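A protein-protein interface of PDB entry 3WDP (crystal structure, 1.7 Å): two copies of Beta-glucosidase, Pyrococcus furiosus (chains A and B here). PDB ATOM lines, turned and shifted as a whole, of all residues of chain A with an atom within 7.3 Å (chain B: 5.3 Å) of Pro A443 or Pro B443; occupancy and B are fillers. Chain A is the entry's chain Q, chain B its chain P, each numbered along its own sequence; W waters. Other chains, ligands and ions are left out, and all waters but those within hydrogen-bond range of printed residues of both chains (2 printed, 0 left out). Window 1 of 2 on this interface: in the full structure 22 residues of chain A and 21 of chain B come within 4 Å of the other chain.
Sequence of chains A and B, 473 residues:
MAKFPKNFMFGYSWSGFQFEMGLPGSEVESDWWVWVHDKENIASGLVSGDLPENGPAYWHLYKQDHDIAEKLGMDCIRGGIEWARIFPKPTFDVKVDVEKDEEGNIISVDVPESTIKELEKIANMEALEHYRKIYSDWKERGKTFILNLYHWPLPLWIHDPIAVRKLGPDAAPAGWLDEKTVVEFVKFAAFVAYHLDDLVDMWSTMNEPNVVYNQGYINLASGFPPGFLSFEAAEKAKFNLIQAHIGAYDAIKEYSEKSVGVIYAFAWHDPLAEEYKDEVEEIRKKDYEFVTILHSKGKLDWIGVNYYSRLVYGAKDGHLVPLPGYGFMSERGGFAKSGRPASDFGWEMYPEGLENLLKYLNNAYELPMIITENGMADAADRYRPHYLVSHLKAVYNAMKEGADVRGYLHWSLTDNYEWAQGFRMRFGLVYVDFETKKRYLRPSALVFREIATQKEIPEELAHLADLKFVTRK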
ATOM      1  N   ALA A 380     -22.357  16.655   3.188  1.00  0.00           N
ATOM      2  CA  ALA A 380     -20.920  16.888   3.427  1.00  0.00           C
ATOM      3  C   ALA A 380     -20.039  15.717   2.977  1.00  0.00           C
ATOM      4  O   ALA A 380     -18.848  15.719   3.227  1.00  0.00           O
ATOM      5  CB  ALA A 380     -20.699  17.139   4.905  1.00  0.00           C
ATOM      6  N   ASP A 381     -20.625  14.703   2.344  1.00  0.00           N
ATOM      7  CA  ASP A 381     -19.877  13.537   1.917  1.00  0.00           C
ATOM      8  C   ASP A 381     -19.264  12.754   3.071  1.00  0.00           C
ATOM      9  O   ASP A 381     -18.251  12.074   2.882  1.00  0.00           O
ATOM     10  CB  ASP A 381     -18.769  13.911   0.920  1.00  0.00           C
ATOM     11  CG  ASP A 381     -18.489  12.828  -0.079  1.00  0.00           C
ATOM     12  OD1 ASP A 381     -19.458  12.394  -0.681  1.00  0.00           O
ATOM     13  OD2 ASP A 381     -17.307  12.431  -0.293  1.00  0.00           O
ATOM     14  N   ARG A 384     -21.036   8.967   2.064  1.00  0.00           N
ATOM     15  CA  ARG A 384     -21.127   8.521   0.653  1.00  0.00           C
ATOM     16  C   ARG A 384     -20.021   7.592   0.189  1.00  0.00           C
ATOM     17  O   ARG A 384     -20.275   6.640  -0.576  1.00  0.00           O
ATOM     18  CB  ARG A 384     -21.165   9.685  -0.297  1.00  0.00           C
ATOM     19  CG  ARG A 384     -21.661   9.271  -1.678  1.00  0.00           C
ATOM     20  CD  ARG A 384     -21.963  10.450  -2.558  1.00  0.00           C
ATOM     21  NE  ARG A 384     -23.200  11.120  -2.209  1.00  0.00           N
ATOM     22  CZ  ARG A 384     -23.315  12.263  -1.540  1.00  0.00           C
ATOM     23  NH1 ARG A 384     -22.255  12.913  -1.068  1.00  0.00           N
ATOM     24  NH2 ARG A 384     -24.509  12.750  -1.320  1.00  0.00           N
ATOM     25  N   PRO A 385     -18.777   7.873   0.608  1.00  0.00           N
ATOM     26  CA  PRO A 385     -17.775   6.908   0.096  1.00  0.00           C
ATOM     27  C   PRO A 385     -18.018   5.482   0.549  1.00  0.00           C
ATOM     28  O   PRO A 385     -17.840   4.536  -0.230  1.00  0.00           O
ATOM     29  CB  PRO A 385     -16.459   7.454   0.687  1.00  0.00           C
ATOM     30  CG  PRO A 385     -16.704   8.935   0.794  1.00  0.00           C
ATOM     31  CD  PRO A 385     -18.150   9.027   1.256  1.00  0.00           C
ATOM     32  N   HIS A 386     -18.389   5.303   1.812  1.00  0.00           N
ATOM     33  CA  HIS A 386     -18.709   3.989   2.320  1.00  0.00           C
ATOM     34  C   HIS A 386     -19.972   3.427   1.626  1.00  0.00           C
ATOM     35  O   HIS A 386     -20.029   2.250   1.269  1.00  0.00           O
ATOM     36  CB  HIS A 386     -18.885   4.006   3.840  1.00  0.00           C
ATOM     37  CG  HIS A 386     -17.604   3.897   4.602  1.00  0.00           C
ATOM     38  ND1 HIS A 386     -16.962   4.998   5.127  1.00  0.00           N
ATOM     39  CD2 HIS A 386     -16.885   2.821   4.999  1.00  0.00           C
ATOM     40  CE1 HIS A 386     -15.874   4.609   5.775  1.00  0.00           C
ATOM     41  NE2 HIS A 386     -15.804   3.294   5.716  1.00  0.00           N
ATOM     42  N   LEU A 388     -21.081   4.165  -1.384  1.00  0.00           N
ATOM     43  CA  LEU A 388     -20.748   3.817  -2.781  1.00  0.00           C
ATOM     44  C   LEU A 388     -20.026   2.452  -2.820  1.00  0.00           C
ATOM     45  O   LEU A 388     -20.457   1.505  -3.510  1.00  0.00           O
ATOM     46  CB  LEU A 388     -19.892   4.903  -3.431  1.00  0.00           C
ATOM     47  CG  LEU A 388     -19.307   4.516  -4.771  1.00  0.00           C
ATOM     48  CD1 LEU A 388     -20.380   4.379  -5.812  1.00  0.00           C
ATOM     49  CD2 LEU A 388     -18.261   5.507  -5.261  1.00  0.00           C
ATOM     50  N   LEU A 429     -22.386  12.971  -6.214  1.00  0.00           N
ATOM     51  CA  LEU A 429     -20.909  12.882  -6.166  1.00  0.00           C
ATOM     52  C   LEU A 429     -20.278  14.283  -6.243  1.00  0.00           C
ATOM     53  O   LEU A 429     -19.105  14.485  -5.849  1.00  0.00           O
ATOM     54  CB  LEU A 429     -20.381  12.047  -7.327  1.00  0.00           C
ATOM     55  CG  LEU A 429     -20.894  10.595  -7.267  1.00  0.00           C
ATOM     56  CD1 LEU A 429     -20.759   9.918  -8.624  1.00  0.00           C
ATOM     57  CD2 LEU A 429     -20.163   9.780  -6.218  1.00  0.00           C
ATOM     58  N   TYR A 440     -18.521  21.410  -7.653  1.00  0.00           N
ATOM     59  CA  TYR A 440     -17.322  21.048  -6.872  1.00  0.00           C
ATOM     60  C   TYR A 440     -17.329  19.546  -6.571  1.00  0.00           C
ATOM     61  O   TYR A 440     -18.328  19.013  -6.110  1.00  0.00           O
ATOM     62  CB  TYR A 440     -17.294  21.823  -5.561  1.00  0.00           C
ATOM     63  CG  TYR A 440     -17.351  23.314  -5.737  1.00  0.00           C
ATOM     64  CD1 TYR A 440     -18.583  23.987  -5.834  1.00  0.00           C
ATOM     65  CD2 TYR A 440     -16.194  24.056  -5.800  1.00  0.00           C
ATOM     66  CE1 TYR A 440     -18.629  25.356  -5.988  1.00  0.00           C
ATOM     67  CE2 TYR A 440     -16.233  25.422  -5.950  1.00  0.00           C
ATOM     68  CZ  TYR A 440     -17.449  26.067  -6.035  1.00  0.00           C
ATOM     69  OH  TYR A 440     -17.485  27.450  -6.228  1.00  0.00           O
ATOM     70  N   LEU A 441     -16.217  18.870  -6.837  1.00  0.00           N
ATOM     71  CA  LEU A 441     -16.114  17.426  -6.516  1.00  0.00           C
ATOM     72  C   LEU A 441     -16.171  17.164  -5.034  1.00  0.00           C
ATOM     73  O   LEU A 441     -15.602  17.909  -4.256  1.00  0.00           O
ATOM     74  CB  LEU A 441     -14.809  16.848  -7.013  1.00  0.00           C
ATOM     75  CG  LEU A 441     -14.514  16.881  -8.495  1.00  0.00           C
ATOM     76  CD1 LEU A 441     -13.291  16.028  -8.735  1.00  0.00           C
ATOM     77  CD2 LEU A 441     -15.712  16.425  -9.327  1.00  0.00           C
ATOM     78  N   ARG A 442     -16.867  16.091  -4.648  1.00  0.00           N
ATOM     79  CA  ARG A 442     -16.751  15.509  -3.316  1.00  0.00           C
ATOM     80  C   ARG A 442     -15.753  14.371  -3.382  1.00  0.00           C
ATOM     81  O   ARG A 442     -15.495  13.840  -4.452  1.00  0.00           O
ATOM     82  CB  ARG A 442     -18.103  15.024  -2.834  1.00  0.00           C
ATOM     83  CG  ARG A 442     -19.110  16.132  -2.634  1.00  0.00           C
ATOM     84  CD  ARG A 442     -20.407  15.631  -2.057  1.00  0.00           C
ATOM     85  NE  ARG A 442     -21.243  16.747  -1.652  1.00  0.00           N
ATOM     86  CZ  ARG A 442     -22.460  17.053  -2.100  1.00  0.00           C
ATOM     87  NH1 ARG A 442     -23.132  16.264  -2.996  1.00  0.00           N
ATOM     88  NH2 ARG A 442     -23.049  18.156  -1.586  1.00  0.00           N
ATOM     89  N   PRO A 443     -15.112  14.039  -2.248  1.00  0.00           N
ATOM     90  CA  PRO A 443     -14.191  12.903  -2.261  1.00  0.00           C
ATOM     91  C   PRO A 443     -14.761  11.581  -2.834  1.00  0.00           C
ATOM     92  O   PRO A 443     -14.021  10.828  -3.468  1.00  0.00           O
ATOM     93  CB  PRO A 443     -13.805  12.747  -0.789  1.00  0.00           C
ATOM     94  CG  PRO A 443     -13.867  14.165  -0.273  1.00  0.00           C
ATOM     95  CD  PRO A 443     -15.106  14.748  -0.949  1.00  0.00           C
ATOM     96  N   SER A 444     -16.041  11.311  -2.600  1.00  0.00           N
ATOM     97  CA  SER A 444     -16.695  10.146  -3.227  1.00  0.00           C
ATOM     98  C   SER A 444     -16.549  10.139  -4.748  1.00  0.00           C
ATOM     99  O   SER A 444     -16.477   9.055  -5.367  1.00  0.00           O
ATOM    100  CB  SER A 444     -18.171  10.113  -2.869  1.00  0.00           C
ATOM    101  OG  SER A 444     -18.783  11.326  -3.176  1.00  0.00           O
ATOM    102  N   ALA A 445     -16.555  11.313  -5.361  1.00  0.00           N
ATOM    103  CA  ALA A 445     -16.281  11.386  -6.813  1.00  0.00           C
ATOM    104  C   ALA A 445     -14.907  10.808  -7.184  1.00  0.00           C
ATOM    105  O   ALA A 445     -14.745  10.119  -8.208  1.00  0.00           O
ATOM    106  CB  ALA A 445     -16.417  12.829  -7.321  1.00  0.00           C
ATOM    107  N   LEU A 446     -13.895  11.088  -6.357  1.00  0.00           N
ATOM    108  CA  LEU A 446     -12.560  10.576  -6.642  1.00  0.00           C
ATOM    109  C   LEU A 446     -12.515   9.050  -6.431  1.00  0.00           C
ATOM    110  O   LEU A 446     -11.811   8.331  -7.136  1.00  0.00           O
ATOM    111  CB  LEU A 446     -11.546  11.257  -5.744  1.00  0.00           C
ATOM    112  CG  LEU A 446     -11.493  12.771  -5.833  1.00  0.00           C
ATOM    113  CD1 LEU A 446     -10.495  13.295  -4.825  1.00  0.00           C
ATOM    114  CD2 LEU A 446     -11.066  13.211  -7.221  1.00  0.00           C
ATOM    115  N   VAL A 447     -13.285   8.555  -5.470  1.00  0.00           N
ATOM    116  CA  VAL A 447     -13.370   7.132  -5.210  1.00  0.00           C
ATOM    117  C   VAL A 447     -14.030   6.456  -6.401  1.00  0.00           C
ATOM    118  O   VAL A 447     -13.547   5.419  -6.903  1.00  0.00           O
ATOM    119  CB  VAL A 447     -14.171   6.848  -3.931  1.00  0.00           C
ATOM    120  CG1 VAL A 447     -14.462   5.352  -3.786  1.00  0.00           C
ATOM    121  CG2 VAL A 447     -13.387   7.363  -2.724  1.00  0.00           C
ATOM    122  N   PHE A 448     -15.123   7.066  -6.856  1.00  0.00           N
ATOM    123  CA  PHE A 448     -15.838   6.577  -8.043  1.00  0.00           C
ATOM    124  C   PHE A 448     -14.897   6.480  -9.230  1.00  0.00           C
ATOM    125  O   PHE A 448     -14.849   5.448  -9.915  1.00  0.00           O
ATOM    126  CB  PHE A 448     -17.050   7.457  -8.365  1.00  0.00           C
ATOM    127  CG  PHE A 448     -17.943   6.883  -9.438  1.00  0.00           C
ATOM    128  CD1 PHE A 448     -17.548   6.860 -10.782  1.00  0.00           C
ATOM    129  CD2 PHE A 448     -19.179   6.352  -9.094  1.00  0.00           C
ATOM    130  CE1 PHE A 448     -18.388   6.298 -11.744  1.00  0.00           C
ATOM    131  CE2 PHE A 448     -20.017   5.831 -10.065  1.00  0.00           C
ATOM    132  CZ  PHE A 448     -19.611   5.793 -11.373  1.00  0.00           C
ATOM    133  N   ARG A 449     -14.123   7.532  -9.469  1.00  0.00           N
ATOM    134  CA  ARG A 449     -13.218   7.576 -10.619  1.00  0.00           C
ATOM    135  C   ARG A 449     -12.220   6.436 -10.561  1.00  0.00           C
ATOM    136  O   ARG A 449     -11.962   5.800 -11.566  1.00  0.00           O
ATOM    137  CB  ARG A 449     -12.509   8.926 -10.721  1.00  0.00           C
ATOM    138  CG  ARG A 449     -11.369   8.924 -11.728  1.00  0.00           C
ATOM    139  CD  ARG A 449     -11.039  10.295 -12.218  1.00  0.00           C
ATOM    140  NE  ARG A 449     -10.497  11.163 -11.198  1.00  0.00           N
ATOM    141  CZ  ARG A 449     -10.561  12.498 -11.218  1.00  0.00           C
ATOM    142  NH1 ARG A 449     -11.187  13.158 -12.190  1.00  0.00           N
ATOM    143  NH2 ARG A 449     -10.004  13.186 -10.240  1.00  0.00           N
ATOM    144  N   LEU A 461      -8.911   0.218  -1.869  1.00  0.00           N
ATOM    145  CA  LEU A 461     -10.207   0.819  -1.545  1.00  0.00           C
ATOM    146  C   LEU A 461     -11.173  -0.177  -0.913  1.00  0.00           C
ATOM    147  O   LEU A 461     -12.308   0.173  -0.617  1.00  0.00           O
ATOM    148  CB  LEU A 461     -10.858   1.421  -2.809  1.00  0.00           C
ATOM    149  CG  LEU A 461     -10.109   2.560  -3.487  1.00  0.00           C
ATOM    150  CD1 LEU A 461     -10.872   3.004  -4.737  1.00  0.00           C
ATOM    151  CD2 LEU A 461      -9.932   3.708  -2.509  1.00  0.00           C
ATOM    152  N   LEU A 464     -13.425   0.454   2.284  1.00  0.00           N
ATOM    153  CA  LEU A 464     -14.618   1.307   2.174  1.00  0.00           C
ATOM    154  C   LEU A 464     -15.912   0.475   2.070  1.00  0.00           C
ATOM    155  O   LEU A 464     -17.006   1.004   2.313  1.00  0.00           O
ATOM    156  CB  LEU A 464     -14.484   2.273   0.997  1.00  0.00           C
ATOM    157  CG  LEU A 464     -13.627   3.525   1.225  1.00  0.00           C
ATOM    158  CD1 LEU A 464     -13.258   4.136  -0.101  1.00  0.00           C
ATOM    159  CD2 LEU A 464     -14.339   4.534   2.114  1.00  0.00           C
ATOM    160  N   ASP B 381     -12.945   8.524   8.276  1.00  0.00           N
ATOM    161  CA  ASP B 381     -12.703   9.566   7.289  1.00  0.00           C
ATOM    162  C   ASP B 381     -13.926  10.451   6.997  1.00  0.00           C
ATOM    163  O   ASP B 381     -14.049  11.012   5.892  1.00  0.00           O
ATOM    164  CB  ASP B 381     -12.180   8.966   5.979  1.00  0.00           C
ATOM    165  CG  ASP B 381     -11.255   9.888   5.231  1.00  0.00           C
ATOM    166  OD1 ASP B 381     -10.292  10.333   5.858  1.00  0.00           O
ATOM    167  OD2 ASP B 381     -11.453  10.124   4.015  1.00  0.00           O
ATOM    168  N   PRO B 385     -11.344  14.914   5.086  1.00  0.00           N
ATOM    169  CA  PRO B 385     -11.132  15.698   3.864  1.00  0.00           C
ATOM    170  C   PRO B 385     -11.357  17.190   4.066  1.00  0.00           C
ATOM    171  O   PRO B 385     -10.621  18.006   3.513  1.00  0.00           O
ATOM    172  CB  PRO B 385     -12.183  15.105   2.905  1.00  0.00           C
ATOM    173  CG  PRO B 385     -12.329  13.685   3.358  1.00  0.00           C
ATOM    174  CD  PRO B 385     -12.250  13.778   4.872  1.00  0.00           C
ATOM    175  N   LEU B 441      -6.278   2.851   1.632  1.00  0.00           N
ATOM    176  CA  LEU B 441      -6.493   4.297   1.461  1.00  0.00           C
ATOM    177  C   LEU B 441      -7.829   4.757   1.984  1.00  0.00           C
ATOM    178  O   LEU B 441      -8.826   4.062   1.828  1.00  0.00           O
ATOM    179  CB  LEU B 441      -6.445   4.672   0.002  1.00  0.00           C
ATOM    180  CG  LEU B 441      -5.150   4.493  -0.753  1.00  0.00           C
ATOM    181  CD1 LEU B 441      -5.309   5.139  -2.102  1.00  0.00           C
ATOM    182  CD2 LEU B 441      -3.948   5.033   0.006  1.00  0.00           C
ATOM    183  N   ARG B 442      -7.847   5.945   2.592  1.00  0.00           N
ATOM    184  CA  ARG B 442      -9.084   6.682   2.847  1.00  0.00           C
ATOM    185  C   ARG B 442      -9.260   7.718   1.763  1.00  0.00           C
ATOM    186  O   ARG B 442      -8.307   8.065   1.080  1.00  0.00           O
ATOM    187  CB  ARG B 442      -9.047   7.333   4.219  1.00  0.00           C
ATOM    188  CG  ARG B 442      -8.972   6.338   5.354  1.00  0.00           C
ATOM    189  CD  ARG B 442      -8.991   7.018   6.698  1.00  0.00           C
ATOM    190  NE  ARG B 442      -9.182   6.052   7.756  1.00  0.00           N
ATOM    191  CZ  ARG B 442      -8.374   5.803   8.792  1.00  0.00           C
ATOM    192  NH1 ARG B 442      -7.264   6.550   9.034  1.00  0.00           N
ATOM    193  NH2 ARG B 442      -8.734   4.830   9.647  1.00  0.00           N
ATOM    194  N   PRO B 443     -10.515   8.151   1.517  1.00  0.00           N
ATOM    195  CA  PRO B 443     -10.745   9.180   0.506  1.00  0.00           C
ATOM    196  C   PRO B 443      -9.891  10.453   0.690  1.00  0.00           C
ATOM    197  O   PRO B 443      -9.488  11.045  -0.297  1.00  0.00           O
ATOM    198  CB  PRO B 443     -12.225   9.499   0.658  1.00  0.00           C
ATOM    199  CG  PRO B 443     -12.824   8.181   1.104  1.00  0.00           C
ATOM    200  CD  PRO B 443     -11.778   7.576   2.029  1.00  0.00           C
ATOM    201  N   SER B 444      -9.612  10.848   1.921  1.00  0.00           N
ATOM    202  CA  SER B 444      -8.717  11.994   2.132  1.00  0.00           C
ATOM    203  C   SER B 444      -7.346  11.787   1.493  1.00  0.00           C
ATOM    204  O   SER B 444      -6.693  12.763   1.100  1.00  0.00           O
ATOM    205  CB  SER B 444      -8.529  12.239   3.616  1.00  0.00           C
ATOM    206  OG  SER B 444      -8.178  11.040   4.238  1.00  0.00           O
ATOM    207  N   ALA B 445      -6.867  10.547   1.455  1.00  0.00           N
ATOM    208  CA  ALA B 445      -5.607  10.268   0.738  1.00  0.00           C
ATOM    209  C   ALA B 445      -5.685  10.657  -0.761  1.00  0.00           C
ATOM    210  O   ALA B 445      -4.722  11.177  -1.359  1.00  0.00           O
ATOM    211  CB  ALA B 445      -5.222   8.789   0.903  1.00  0.00           C
ATOM    212  N   LEU B 446      -6.835  10.387  -1.392  1.00  0.00           N
ATOM    213  CA  LEU B 446      -7.017  10.750  -2.794  1.00  0.00           C
ATOM    214  C   LEU B 446      -7.077  12.274  -2.965  1.00  0.00           C
ATOM    215  O   LEU B 446      -6.562  12.838  -3.928  1.00  0.00           O
ATOM    216  CB  LEU B 446      -8.269  10.101  -3.355  1.00  0.00           C
ATOM    217  CG  LEU B 446      -8.344   8.583  -3.253  1.00  0.00           C
ATOM    218  CD1 LEU B 446      -9.636   8.112  -3.880  1.00  0.00           C
ATOM    219  CD2 LEU B 446      -7.178   7.928  -3.957  1.00  0.00           C
ATOM    220  N   VAL B 447      -7.673  12.948  -1.998  1.00  0.00           N
ATOM    221  CA  VAL B 447      -7.741  14.396  -2.008  1.00  0.00           C
ATOM    222  C   VAL B 447      -6.349  14.976  -1.869  1.00  0.00           C
ATOM    223  O   VAL B 447      -5.964  15.913  -2.603  1.00  0.00           O
ATOM    224  CB  VAL B 447      -8.645  14.892  -0.866  1.00  0.00           C
ATOM    225  CG1 VAL B 447      -8.528  16.413  -0.648  1.00  0.00           C
ATOM    226  CG2 VAL B 447     -10.091  14.464  -1.164  1.00  0.00           C
ATOM    227  N   PHE B 448      -5.599  14.419  -0.913  1.00  0.00           N
ATOM    228  CA  PHE B 448      -4.209  14.842  -0.697  1.00  0.00           C
ATOM    229  C   PHE B 448      -3.409  14.676  -1.989  1.00  0.00           C
ATOM    230  O   PHE B 448      -2.708  15.593  -2.414  1.00  0.00           O
ATOM    231  CB  PHE B 448      -3.586  14.078   0.481  1.00  0.00           C
ATOM    232  CG  PHE B 448      -2.205  14.560   0.858  1.00  0.00           C
ATOM    233  CD1 PHE B 448      -1.107  14.363   0.010  1.00  0.00           C
ATOM    234  CD2 PHE B 448      -2.016  15.214   2.061  1.00  0.00           C
ATOM    235  CE1 PHE B 448       0.155  14.840   0.385  1.00  0.00           C
ATOM    236  CE2 PHE B 448      -0.750  15.652   2.439  1.00  0.00           C
ATOM    237  CZ  PHE B 448       0.312  15.480   1.580  1.00  0.00           C
ATOM    238  N   LEU B 464     -14.137  21.969  -0.275  1.00  0.00           N
ATOM    239  CA  LEU B 464     -13.676  21.231   0.908  1.00  0.00           C
ATOM    240  C   LEU B 464     -13.075  22.156   1.982  1.00  0.00           C
ATOM    241  O   LEU B 464     -12.963  21.763   3.149  1.00  0.00           O
ATOM    242  CB  LEU B 464     -12.704  20.134   0.497  1.00  0.00           C
ATOM    243  CG  LEU B 464     -13.346  18.849  -0.066  1.00  0.00           C
ATOM    244  CD1 LEU B 464     -12.293  18.028  -0.742  1.00  0.00           C
ATOM    245  CD2 LEU B 464     -14.055  18.050   1.018  1.00  0.00           C
HETATM  246  O   HOH W   1     -10.270   1.319   1.710  1.00  0.00           O
HETATM  247  O   HOH W   2     -14.791  20.782  -3.265  1.00  0.00           O
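Among the printed residues, pairs that only touch across the chains: Pro A385 with Pro B443 (3.7 Å), Pro A443 with Pro B385 (3.7 Å), Pro A443 with Pro B443 (3.9 Å), Pro A443 with Val B447 (3.9 Å), Pro A443 with Leu B464 (3.98 Å), Leu A446 with Leu B446 (3.9 Å), Leu A446 with Val B447 (3.9 Å), Val A447 with Pro B443 (3.95 Å), Val A447 with Leu B446 (3.996 Å) and Leu A464 with Pro B443 (3.98 Å).
Of the printed residues of chain B, Pro A443 touches Pro B385, Pro B443, Val B447 and Leu B464.
Of the printed residues of chain A, Val B447 touches Pro A443 and Leu A446.
Printed residues of chain B within 4 Å of Pro A385: Pro B443.
Printed residues of chain A within 4 Å of Leu B464: Pro A443 (3.98 Å).
Arg A442 touches none of the printed residues of chain B.
Leu A429 touches none of the printed residues of chain B.
The nearest residue of chain A that does not touch Pro B443 is Leu A446 (5.2 Å).
Of the 19 printed residues of chain A, 5 touch a printed residue of chain B.
Printed residues of chain A that touch a printed residue of chain B: Pro A385, Pro A443, Leu A446, Val A447 and Leu A464.
Hydrophobic or aromatic side chains of chain A within 4 Å of the printed part of chain B: Pro A385, Pro A443, Leu A446, Val A447 and Leu A464.
Of the 11 printed residues of chain B, 5 touch a printed residue of chain A.
Hydrophobic or aromatic side chains of chain B that line the printed part of chain A: Pro B385, Pro B443, Leu B446, Val B447 and Leu B464.
Pro A385 touches Pro B443, and with the chains exchanged Pro A443 touches Pro B385.
Pro B443 touches its own counterpart, Pro A443.
Leu A446 touches its own counterpart, Leu B446.
Leu A446 touches Val B447, and with the chains exchanged Val A447 touches Leu B446.
Water W1 lies within hydrogen-bond range of O of Leu B441 (3.1 Å), O of Leu A461 (3.3 Å) and N of Leu A464 (3.3 Å).
Water W2 lies within hydrogen-bond range of O of Leu A441 (3.1 Å) and N of Leu B464 (3.3 Å).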
